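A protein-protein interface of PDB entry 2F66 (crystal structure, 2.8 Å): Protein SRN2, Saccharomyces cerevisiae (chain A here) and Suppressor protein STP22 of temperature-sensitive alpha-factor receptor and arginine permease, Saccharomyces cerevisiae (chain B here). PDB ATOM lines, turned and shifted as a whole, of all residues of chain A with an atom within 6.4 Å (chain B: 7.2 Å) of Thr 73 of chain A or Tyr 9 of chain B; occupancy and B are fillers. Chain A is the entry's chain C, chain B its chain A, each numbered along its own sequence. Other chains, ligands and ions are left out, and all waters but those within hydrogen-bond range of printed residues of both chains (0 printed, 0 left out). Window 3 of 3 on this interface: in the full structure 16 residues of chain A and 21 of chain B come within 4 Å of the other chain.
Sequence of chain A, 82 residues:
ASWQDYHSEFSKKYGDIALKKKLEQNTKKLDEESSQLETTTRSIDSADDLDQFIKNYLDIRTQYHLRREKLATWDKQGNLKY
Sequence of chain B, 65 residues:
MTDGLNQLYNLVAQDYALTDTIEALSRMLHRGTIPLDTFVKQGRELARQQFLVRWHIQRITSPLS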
ATOM      1  N   LYS A  20      -3.729  11.857 -31.348  1.00  0.00           N
ATOM      2  CA  LYS A  20      -4.357  10.811 -30.551  1.00  0.00           C
ATOM      3  C   LYS A  20      -3.275   9.869 -30.055  1.00  0.00           C
ATOM      4  O   LYS A  20      -3.218   9.525 -28.878  1.00  0.00           O
ATOM      5  CB  LYS A  20      -5.342   9.998 -31.388  1.00  0.00           C
ATOM      6  CG  LYS A  20      -6.679  10.648 -31.639  1.00  0.00           C
ATOM      7  CD  LYS A  20      -7.511   9.756 -32.545  1.00  0.00           C
ATOM      8  CE  LYS A  20      -8.936  10.248 -32.668  1.00  0.00           C
ATOM      9  NZ  LYS A  20      -9.634  10.137 -31.362  1.00  0.00           N
ATOM     10  N   HIS A  65      -7.351  10.088 -15.940  1.00  0.00           N
ATOM     11  CA  HIS A  65      -8.731  10.047 -16.402  1.00  0.00           C
ATOM     12  C   HIS A  65      -9.066  11.206 -17.317  1.00  0.00           C
ATOM     13  O   HIS A  65      -9.840  11.048 -18.256  1.00  0.00           O
ATOM     14  CB  HIS A  65      -9.695  10.033 -15.218  1.00  0.00           C
ATOM     15  CG  HIS A  65      -9.730   8.727 -14.494  1.00  0.00           C
ATOM     16  ND1 HIS A  65     -10.248   7.582 -15.058  1.00  0.00           N
ATOM     17  CD2 HIS A  65      -9.271   8.371 -13.270  1.00  0.00           C
ATOM     18  CE1 HIS A  65     -10.106   6.575 -14.213  1.00  0.00           C
ATOM     19  NE2 HIS A  65      -9.515   7.028 -13.122  1.00  0.00           N
ATOM     20  N   LEU A  66      -8.488  12.372 -17.058  1.00  0.00           N
ATOM     21  CA  LEU A  66      -8.776  13.517 -17.906  1.00  0.00           C
ATOM     22  C   LEU A  66      -8.452  13.200 -19.360  1.00  0.00           C
ATOM     23  O   LEU A  66      -9.331  13.240 -20.221  1.00  0.00           O
ATOM     24  CB  LEU A  66      -7.990  14.748 -17.445  1.00  0.00           C
ATOM     25  CG  LEU A  66      -8.278  16.060 -18.190  1.00  0.00           C
ATOM     26  CD1 LEU A  66      -9.774  16.212 -18.444  1.00  0.00           C
ATOM     27  CD2 LEU A  66      -7.751  17.231 -17.371  1.00  0.00           C
ATOM     28  N   ARG A  68      -7.810  10.435 -20.538  1.00  0.00           N
ATOM     29  CA  ARG A  68      -8.547   9.217 -20.815  1.00  0.00           C
ATOM     30  C   ARG A  68      -9.916   9.568 -21.412  1.00  0.00           C
ATOM     31  O   ARG A  68     -10.373   8.935 -22.369  1.00  0.00           O
ATOM     32  CB  ARG A  68      -8.711   8.432 -19.509  1.00  0.00           C
ATOM     33  CG  ARG A  68      -8.955   6.947 -19.666  1.00  0.00           C
ATOM     34  CD  ARG A  68      -7.732   6.227 -20.194  1.00  0.00           C
ATOM     35  NE  ARG A  68      -7.963   4.791 -20.351  1.00  0.00           N
ATOM     36  CZ  ARG A  68      -8.982   4.253 -21.022  1.00  0.00           C
ATOM     37  NH1 ARG A  68      -9.891   5.025 -21.609  1.00  0.00           N
ATOM     38  NH2 ARG A  68      -9.088   2.934 -21.119  1.00  0.00           N
ATOM     39  N   GLU A  69     -10.568  10.582 -20.854  1.00  0.00           N
ATOM     40  CA  GLU A  69     -11.879  10.969 -21.350  1.00  0.00           C
ATOM     41  C   GLU A  69     -11.772  11.926 -22.514  1.00  0.00           C
ATOM     42  O   GLU A  69     -12.655  11.983 -23.361  1.00  0.00           O
ATOM     43  CB  GLU A  69     -12.745  11.565 -20.222  1.00  0.00           C
ATOM     44  CG  GLU A  69     -12.094  12.634 -19.370  1.00  0.00           C
ATOM     45  CD  GLU A  69     -12.739  12.744 -17.996  1.00  0.00           C
ATOM     46  OE1 GLU A  69     -12.855  11.707 -17.312  1.00  0.00           O
ATOM     47  OE2 GLU A  69     -13.123  13.859 -17.593  1.00  0.00           O
ATOM     48  N   LYS A  70     -10.676  12.664 -22.569  1.00  0.00           N
ATOM     49  CA  LYS A  70     -10.461  13.609 -23.657  1.00  0.00           C
ATOM     50  C   LYS A  70     -10.177  12.821 -24.939  1.00  0.00           C
ATOM     51  O   LYS A  70     -10.512  13.249 -26.045  1.00  0.00           O
ATOM     52  CB  LYS A  70      -9.263  14.499 -23.336  1.00  0.00           C
ATOM     53  CG  LYS A  70      -9.290  15.831 -24.036  1.00  0.00           C
ATOM     54  CD  LYS A  70      -9.723  16.948 -23.088  1.00  0.00           C
ATOM     55  CE  LYS A  70      -8.597  17.345 -22.132  1.00  0.00           C
ATOM     56  NZ  LYS A  70      -8.921  18.584 -21.359  1.00  0.00           N
ATOM     57  N   LEU A  71      -9.564  11.656 -24.768  1.00  0.00           N
ATOM     58  CA  LEU A  71      -9.199  10.816 -25.888  1.00  0.00           C
ATOM     59  C   LEU A  71     -10.365  10.056 -26.502  1.00  0.00           C
ATOM     60  O   LEU A  71     -10.530  10.040 -27.721  1.00  0.00           O
ATOM     61  CB  LEU A  71      -8.115   9.830 -25.461  1.00  0.00           C
ATOM     62  CG  LEU A  71      -7.520   8.971 -26.578  1.00  0.00           C
ATOM     63  CD1 LEU A  71      -6.906   9.846 -27.663  1.00  0.00           C
ATOM     64  CD2 LEU A  71      -6.467   8.081 -25.990  1.00  0.00           C
ATOM     65  N   ALA A  72     -11.175   9.417 -25.672  1.00  0.00           N
ATOM     66  CA  ALA A  72     -12.301   8.662 -26.200  1.00  0.00           C
ATOM     67  C   ALA A  72     -13.411   9.596 -26.665  1.00  0.00           C
ATOM     68  O   ALA A  72     -14.428   9.150 -27.196  1.00  0.00           O
ATOM     69  CB  ALA A  72     -12.827   7.707 -25.139  1.00  0.00           C
ATOM     70  N   THR A  73     -13.204  10.895 -26.477  1.00  0.00           N
ATOM     71  CA  THR A  73     -14.202  11.886 -26.858  1.00  0.00           C
ATOM     72  C   THR A  73     -13.654  12.824 -27.937  1.00  0.00           C
ATOM     73  O   THR A  73     -14.309  13.785 -28.352  1.00  0.00           O
ATOM     74  CB  THR A  73     -14.608  12.717 -25.628  1.00  0.00           C
ATOM     75  OG1 THR A  73     -15.829  13.401 -25.898  1.00  0.00           O
ATOM     76  CG2 THR A  73     -13.532  13.750 -25.299  1.00  0.00           C
ATOM     77  N   TRP A  74     -12.442  12.519 -28.384  1.00  0.00           N
ATOM     78  CA  TRP A  74     -11.731  13.303 -29.388  1.00  0.00           C
ATOM     79  C   TRP A  74     -12.553  13.902 -30.527  1.00  0.00           C
ATOM     80  O   TRP A  74     -12.250  14.996 -31.001  1.00  0.00           O
ATOM     81  CB  TRP A  74     -10.595  12.456 -29.973  1.00  0.00           C
ATOM     82  CG  TRP A  74      -9.643  13.239 -30.805  1.00  0.00           C
ATOM     83  CD1 TRP A  74      -9.797  13.598 -32.110  1.00  0.00           C
ATOM     84  CD2 TRP A  74      -8.408  13.819 -30.369  1.00  0.00           C
ATOM     85  NE1 TRP A  74      -8.735  14.371 -32.517  1.00  0.00           N
ATOM     86  CE2 TRP A  74      -7.868  14.523 -31.466  1.00  0.00           C
ATOM     87  CE3 TRP A  74      -7.708  13.815 -29.155  1.00  0.00           C
ATOM     88  CZ2 TRP A  74      -6.653  15.219 -31.388  1.00  0.00           C
ATOM     89  CZ3 TRP A  74      -6.498  14.508 -29.076  1.00  0.00           C
ATOM     90  CH2 TRP A  74      -5.985  15.201 -30.188  1.00  0.00           C
ATOM     91  N   ASP A  75     -13.592  13.203 -30.964  1.00  0.00           N
ATOM     92  CA  ASP A  75     -14.405  13.691 -32.076  1.00  0.00           C
ATOM     93  C   ASP A  75     -15.804  14.159 -31.664  1.00  0.00           C
ATOM     94  O   ASP A  75     -16.141  15.331 -31.951  1.00  0.00           O
ATOM     95  CB  ASP A  75     -14.500  12.592 -33.132  1.00  0.00           C
ATOM     96  CG  ASP A  75     -13.153  11.940 -33.409  1.00  0.00           C
ATOM     97  OD1 ASP A  75     -12.255  12.624 -33.947  1.00  0.00           O
ATOM     98  OD2 ASP A  75     -12.989  10.745 -33.077  1.00  0.00           O
ATOM     99  N   MET B   1     -12.196  23.895 -26.676  1.00  0.00           N
ATOM    100  CA  MET B   1     -12.767  23.497 -25.359  1.00  0.00           C
ATOM    101  C   MET B   1     -13.114  24.723 -24.506  1.00  0.00           C
ATOM    102  O   MET B   1     -12.224  25.387 -23.966  1.00  0.00           O
ATOM    103  CB  MET B   1     -11.764  22.618 -24.607  1.00  0.00           C
ATOM    104  CG  MET B   1     -12.316  21.988 -23.332  1.00  0.00           C
ATOM    105  SD  MET B   1     -13.528  20.674 -23.632  1.00  0.00           S
ATOM    106  CE  MET B   1     -12.499  19.207 -23.376  1.00  0.00           C
ATOM    107  N   ASP B   3     -14.604  27.058 -21.348  1.00  0.00           N
ATOM    108  CA  ASP B   3     -14.179  27.045 -19.953  1.00  0.00           C
ATOM    109  C   ASP B   3     -15.051  26.110 -19.128  1.00  0.00           C
ATOM    110  O   ASP B   3     -14.554  25.342 -18.300  1.00  0.00           O
ATOM    111  CB  ASP B   3     -14.243  28.456 -19.362  1.00  0.00           C
ATOM    112  CG  ASP B   3     -12.917  29.187 -19.452  1.00  0.00           C
ATOM    113  OD1 ASP B   3     -12.410  29.374 -20.578  1.00  0.00           O
ATOM    114  OD2 ASP B   3     -12.381  29.573 -18.391  1.00  0.00           O
ATOM    115  N   GLY B   4     -16.357  26.183 -19.357  1.00  0.00           N
ATOM    116  CA  GLY B   4     -17.279  25.334 -18.632  1.00  0.00           C
ATOM    117  C   GLY B   4     -17.119  23.877 -19.018  1.00  0.00           C
ATOM    118  O   GLY B   4     -17.164  22.988 -18.163  1.00  0.00           O
ATOM    119  N   LEU B   5     -16.931  23.626 -20.308  1.00  0.00           N
ATOM    120  CA  LEU B   5     -16.771  22.264 -20.788  1.00  0.00           C
ATOM    121  C   LEU B   5     -15.481  21.652 -20.245  1.00  0.00           C
ATOM    122  O   LEU B   5     -15.409  20.454 -19.962  1.00  0.00           O
ATOM    123  CB  LEU B   5     -16.757  22.247 -22.311  1.00  0.00           C
ATOM    124  CG  LEU B   5     -16.997  20.867 -22.915  1.00  0.00           C
ATOM    125  CD1 LEU B   5     -18.372  20.356 -22.493  1.00  0.00           C
ATOM    126  CD2 LEU B   5     -16.900  20.954 -24.426  1.00  0.00           C
ATOM    127  N   ASN B   6     -14.459  22.484 -20.097  1.00  0.00           N
ATOM    128  CA  ASN B   6     -13.185  22.018 -19.576  1.00  0.00           C
ATOM    129  C   ASN B   6     -13.374  21.608 -18.124  1.00  0.00           C
ATOM    130  O   ASN B   6     -12.911  20.553 -17.701  1.00  0.00           O
ATOM    131  CB  ASN B   6     -12.143  23.129 -19.671  1.00  0.00           C
ATOM    132  CG  ASN B   6     -10.854  22.655 -20.286  1.00  0.00           C
ATOM    133  OD1 ASN B   6     -10.201  21.748 -19.766  1.00  0.00           O
ATOM    134  ND2 ASN B   6     -10.480  23.261 -21.407  1.00  0.00           N
ATOM    135  N   GLN B   7     -14.056  22.459 -17.366  1.00  0.00           N
ATOM    136  CA  GLN B   7     -14.341  22.211 -15.958  1.00  0.00           C
ATOM    137  C   GLN B   7     -14.999  20.850 -15.783  1.00  0.00           C
ATOM    138  O   GLN B   7     -14.563  20.026 -14.985  1.00  0.00           O
ATOM    139  CB  GLN B   7     -15.294  23.272 -15.436  1.00  0.00           C
ATOM    140  CG  GLN B   7     -15.539  23.192 -13.951  1.00  0.00           C
ATOM    141  CD  GLN B   7     -16.613  24.162 -13.498  1.00  0.00           C
ATOM    142  OE1 GLN B   7     -16.697  24.506 -12.317  1.00  0.00           O
ATOM    143  NE2 GLN B   7     -17.453  24.598 -14.432  1.00  0.00           N
ATOM    144  N   LEU B   8     -16.064  20.635 -16.542  1.00  0.00           N
ATOM    145  CA  LEU B   8     -16.815  19.403 -16.500  1.00  0.00           C
ATOM    146  C   LEU B   8     -15.884  18.208 -16.627  1.00  0.00           C
ATOM    147  O   LEU B   8     -15.976  17.243 -15.868  1.00  0.00           O
ATOM    148  CB  LEU B   8     -17.843  19.404 -17.631  1.00  0.00           C
ATOM    149  CG  LEU B   8     -18.817  18.231 -17.690  1.00  0.00           C
ATOM    150  CD1 LEU B   8     -19.558  18.129 -16.376  1.00  0.00           C
ATOM    151  CD2 LEU B   8     -19.790  18.428 -18.844  1.00  0.00           C
ATOM    152  N   TYR B   9     -14.977  18.275 -17.588  1.00  0.00           N
ATOM    153  CA  TYR B   9     -14.044  17.182 -17.805  1.00  0.00           C
ATOM    154  C   TYR B   9     -13.177  16.910 -16.587  1.00  0.00           C
ATOM    155  O   TYR B   9     -12.900  15.758 -16.264  1.00  0.00           O
ATOM    156  CB  TYR B   9     -13.156  17.476 -19.018  1.00  0.00           C
ATOM    157  CG  TYR B   9     -13.703  16.964 -20.333  1.00  0.00           C
ATOM    158  CD1 TYR B   9     -14.862  17.498 -20.885  1.00  0.00           C
ATOM    159  CD2 TYR B   9     -13.042  15.951 -21.034  1.00  0.00           C
ATOM    160  CE1 TYR B   9     -15.348  17.043 -22.109  1.00  0.00           C
ATOM    161  CE2 TYR B   9     -13.519  15.488 -22.256  1.00  0.00           C
ATOM    162  CZ  TYR B   9     -14.669  16.041 -22.788  1.00  0.00           C
ATOM    163  OH  TYR B   9     -15.132  15.615 -24.009  1.00  0.00           O
ATOM    164  N   ASN B  10     -12.742  17.968 -15.912  1.00  0.00           N
ATOM    165  CA  ASN B  10     -11.903  17.803 -14.735  1.00  0.00           C
ATOM    166  C   ASN B  10     -12.674  17.265 -13.540  1.00  0.00           C
ATOM    167  O   ASN B  10     -12.164  16.429 -12.782  1.00  0.00           O
ATOM    168  CB  ASN B  10     -11.215  19.120 -14.379  1.00  0.00           C
ATOM    169  CG  ASN B  10     -10.046  19.414 -15.290  1.00  0.00           C
ATOM    170  OD1 ASN B  10     -10.225  19.769 -16.457  1.00  0.00           O
ATOM    171  ND2 ASN B  10      -8.836  19.238 -14.770  1.00  0.00           N
ATOM    172  N   LEU B  11     -13.904  17.741 -13.374  1.00  0.00           N
ATOM    173  CA  LEU B  11     -14.744  17.282 -12.282  1.00  0.00           C
ATOM    174  C   LEU B  11     -14.932  15.780 -12.436  1.00  0.00           C
ATOM    175  O   LEU B  11     -14.722  15.018 -11.496  1.00  0.00           O
ATOM    176  CB  LEU B  11     -16.092  18.003 -12.312  1.00  0.00           C
ATOM    177  CG  LEU B  11     -16.020  19.478 -11.896  1.00  0.00           C
ATOM    178  CD1 LEU B  11     -17.422  20.082 -11.907  1.00  0.00           C
ATOM    179  CD2 LEU B  11     -15.401  19.591 -10.505  1.00  0.00           C
ATOM    180  N   VAL B  12     -15.317  15.352 -13.627  1.00  0.00           N
ATOM    181  CA  VAL B  12     -15.491  13.929 -13.879  1.00  0.00           C
ATOM    182  C   VAL B  12     -14.184  13.192 -13.580  1.00  0.00           C
ATOM    183  O   VAL B  12     -14.182  12.155 -12.915  1.00  0.00           O
ATOM    184  CB  VAL B  12     -15.914  13.673 -15.353  1.00  0.00           C
ATOM    185  CG1 VAL B  12     -15.758  12.201 -15.708  1.00  0.00           C
ATOM    186  CG2 VAL B  12     -17.368  14.115 -15.553  1.00  0.00           C
ATOM    187  N   ALA B  13     -13.076  13.746 -14.066  1.00  0.00           N
ATOM    188  CA  ALA B  13     -11.760  13.157 -13.863  1.00  0.00           C
ATOM    189  C   ALA B  13     -11.489  12.974 -12.377  1.00  0.00           C
ATOM    190  O   ALA B  13     -11.002  11.919 -11.946  1.00  0.00           O
ATOM    191  CB  ALA B  13     -10.709  14.042 -14.483  1.00  0.00           C
ATOM    192  N   GLN B  14     -11.809  14.011 -11.603  1.00  0.00           N
ATOM    193  CA  GLN B  14     -11.634  14.009 -10.149  1.00  0.00           C
ATOM    194  C   GLN B  14     -12.489  12.965  -9.426  1.00  0.00           C
ATOM    195  O   GLN B  14     -12.063  12.388  -8.432  1.00  0.00           O
ATOM    196  CB  GLN B  14     -11.980  15.377  -9.594  1.00  0.00           C
ATOM    197  CG  GLN B  14     -10.928  16.417  -9.829  1.00  0.00           C
ATOM    198  CD  GLN B  14     -11.424  17.815  -9.545  1.00  0.00           C
ATOM    199  OE1 GLN B  14     -12.071  18.067  -8.524  1.00  0.00           O
ATOM    200  NE2 GLN B  14     -11.120  18.739 -10.448  1.00  0.00           N
ATOM    201  N   ASP B  15     -13.705  12.747  -9.916  1.00  0.00           N
ATOM    202  CA  ASP B  15     -14.609  11.773  -9.327  1.00  0.00           C
ATOM    203  C   ASP B  15     -13.968  10.394  -9.414  1.00  0.00           C
ATOM    204  O   ASP B  15     -13.802   9.714  -8.398  1.00  0.00           O
ATOM    205  CB  ASP B  15     -15.957  11.787 -10.074  1.00  0.00           C
ATOM    206  CG  ASP B  15     -16.958  10.739  -9.549  1.00  0.00           C
ATOM    207  OD1 ASP B  15     -16.618   9.943  -8.640  1.00  0.00           O
ATOM    208  OD2 ASP B  15     -18.100  10.710 -10.066  1.00  0.00           O
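OG1 of Thr 73 of chain A lies close to OH of Tyr 9 of chain B, at 3.0 Å.
The side-chain carboxylate (OE2) of Glu 69 of chain A lies close to the backbone carbonyl oxygen (O) of Tyr 9 of chain B (2.3 Å).
The backbone carbonyl oxygen of Asn 6 of chain B sits close to the side-chain amide oxygen of Asn 10 of chain B.
The backbone carbonyl oxygen of Asn 10 of chain B sits close to the side-chain amide nitrogen of Gln 14 of chain B, 3.4 Å away.
His 65 of chain A touches Ala 13 of chain B (CB to CA, 3.98 Å).
Leu 66 of chain A touches Tyr 9 of chain B (CD1 to CB, 3.7 Å).
Leu 66 of chain A touches Asn 10 of chain B (CD2 to ND2, 3.5 Å).
Leu 66 of chain A touches Ala 13 of chain B.
Glu 69 of chain A touches Val 12 of chain B (OE1 to CG1, 3.4 Å).
OE2 of Glu 69 of chain A touches N of Ala 13 of chain B, at 3.5 Å.
CD of Lys 70 of chain A touches CE of Met 1 of chain B (3.6 Å).
Lys 70 of chain A touches Asn 6 of chain B (NZ to OD1, 3.8 Å).
Lys 70 of chain A touches Tyr 9 of chain B.
Printed residues of chain B within 4 Å of His 65 of chain A: Ala 13.
Of the printed residues of chain B, Leu 66 of chain A touches Tyr 9 (3.7 Å), Asn 10 (3.5 Å) and Ala 13 (3.8 Å).
Of the printed residues of chain B, Glu 69 of chain A touches Tyr 9 (2.3 Å), Val 12 (3.4 Å) and Ala 13 (3.5 Å).
Of the printed residues of chain B, Lys 70 of chain A touches Met 1 (3.6 Å), Asn 6 (3.8 Å) and Tyr 9 (3.9 Å).
Tyr 9 of chain B touches just these residues of chain A: Leu 66 (3.7 Å), Glu 69 (2.3 Å), Lys 70 (3.9 Å) and Thr 73 (2.8 Å).
Of the printed residues of chain A, Val 12 of chain B touches Glu 69 (3.4 Å).
The nearest residue of chain B that does not touch Thr 73 of chain A is Met 1 of chain B (5.9 Å).
The nearest residue of chain A that does not touch Tyr 9 of chain B is His 65 of chain A (6.0 Å).
Printed residues of chain A that touch a printed residue of chain B: His 65, Leu 66, Glu 69, Lys 70 and Thr 73.
Among the printed residues, 11 pairs touch across the chains.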
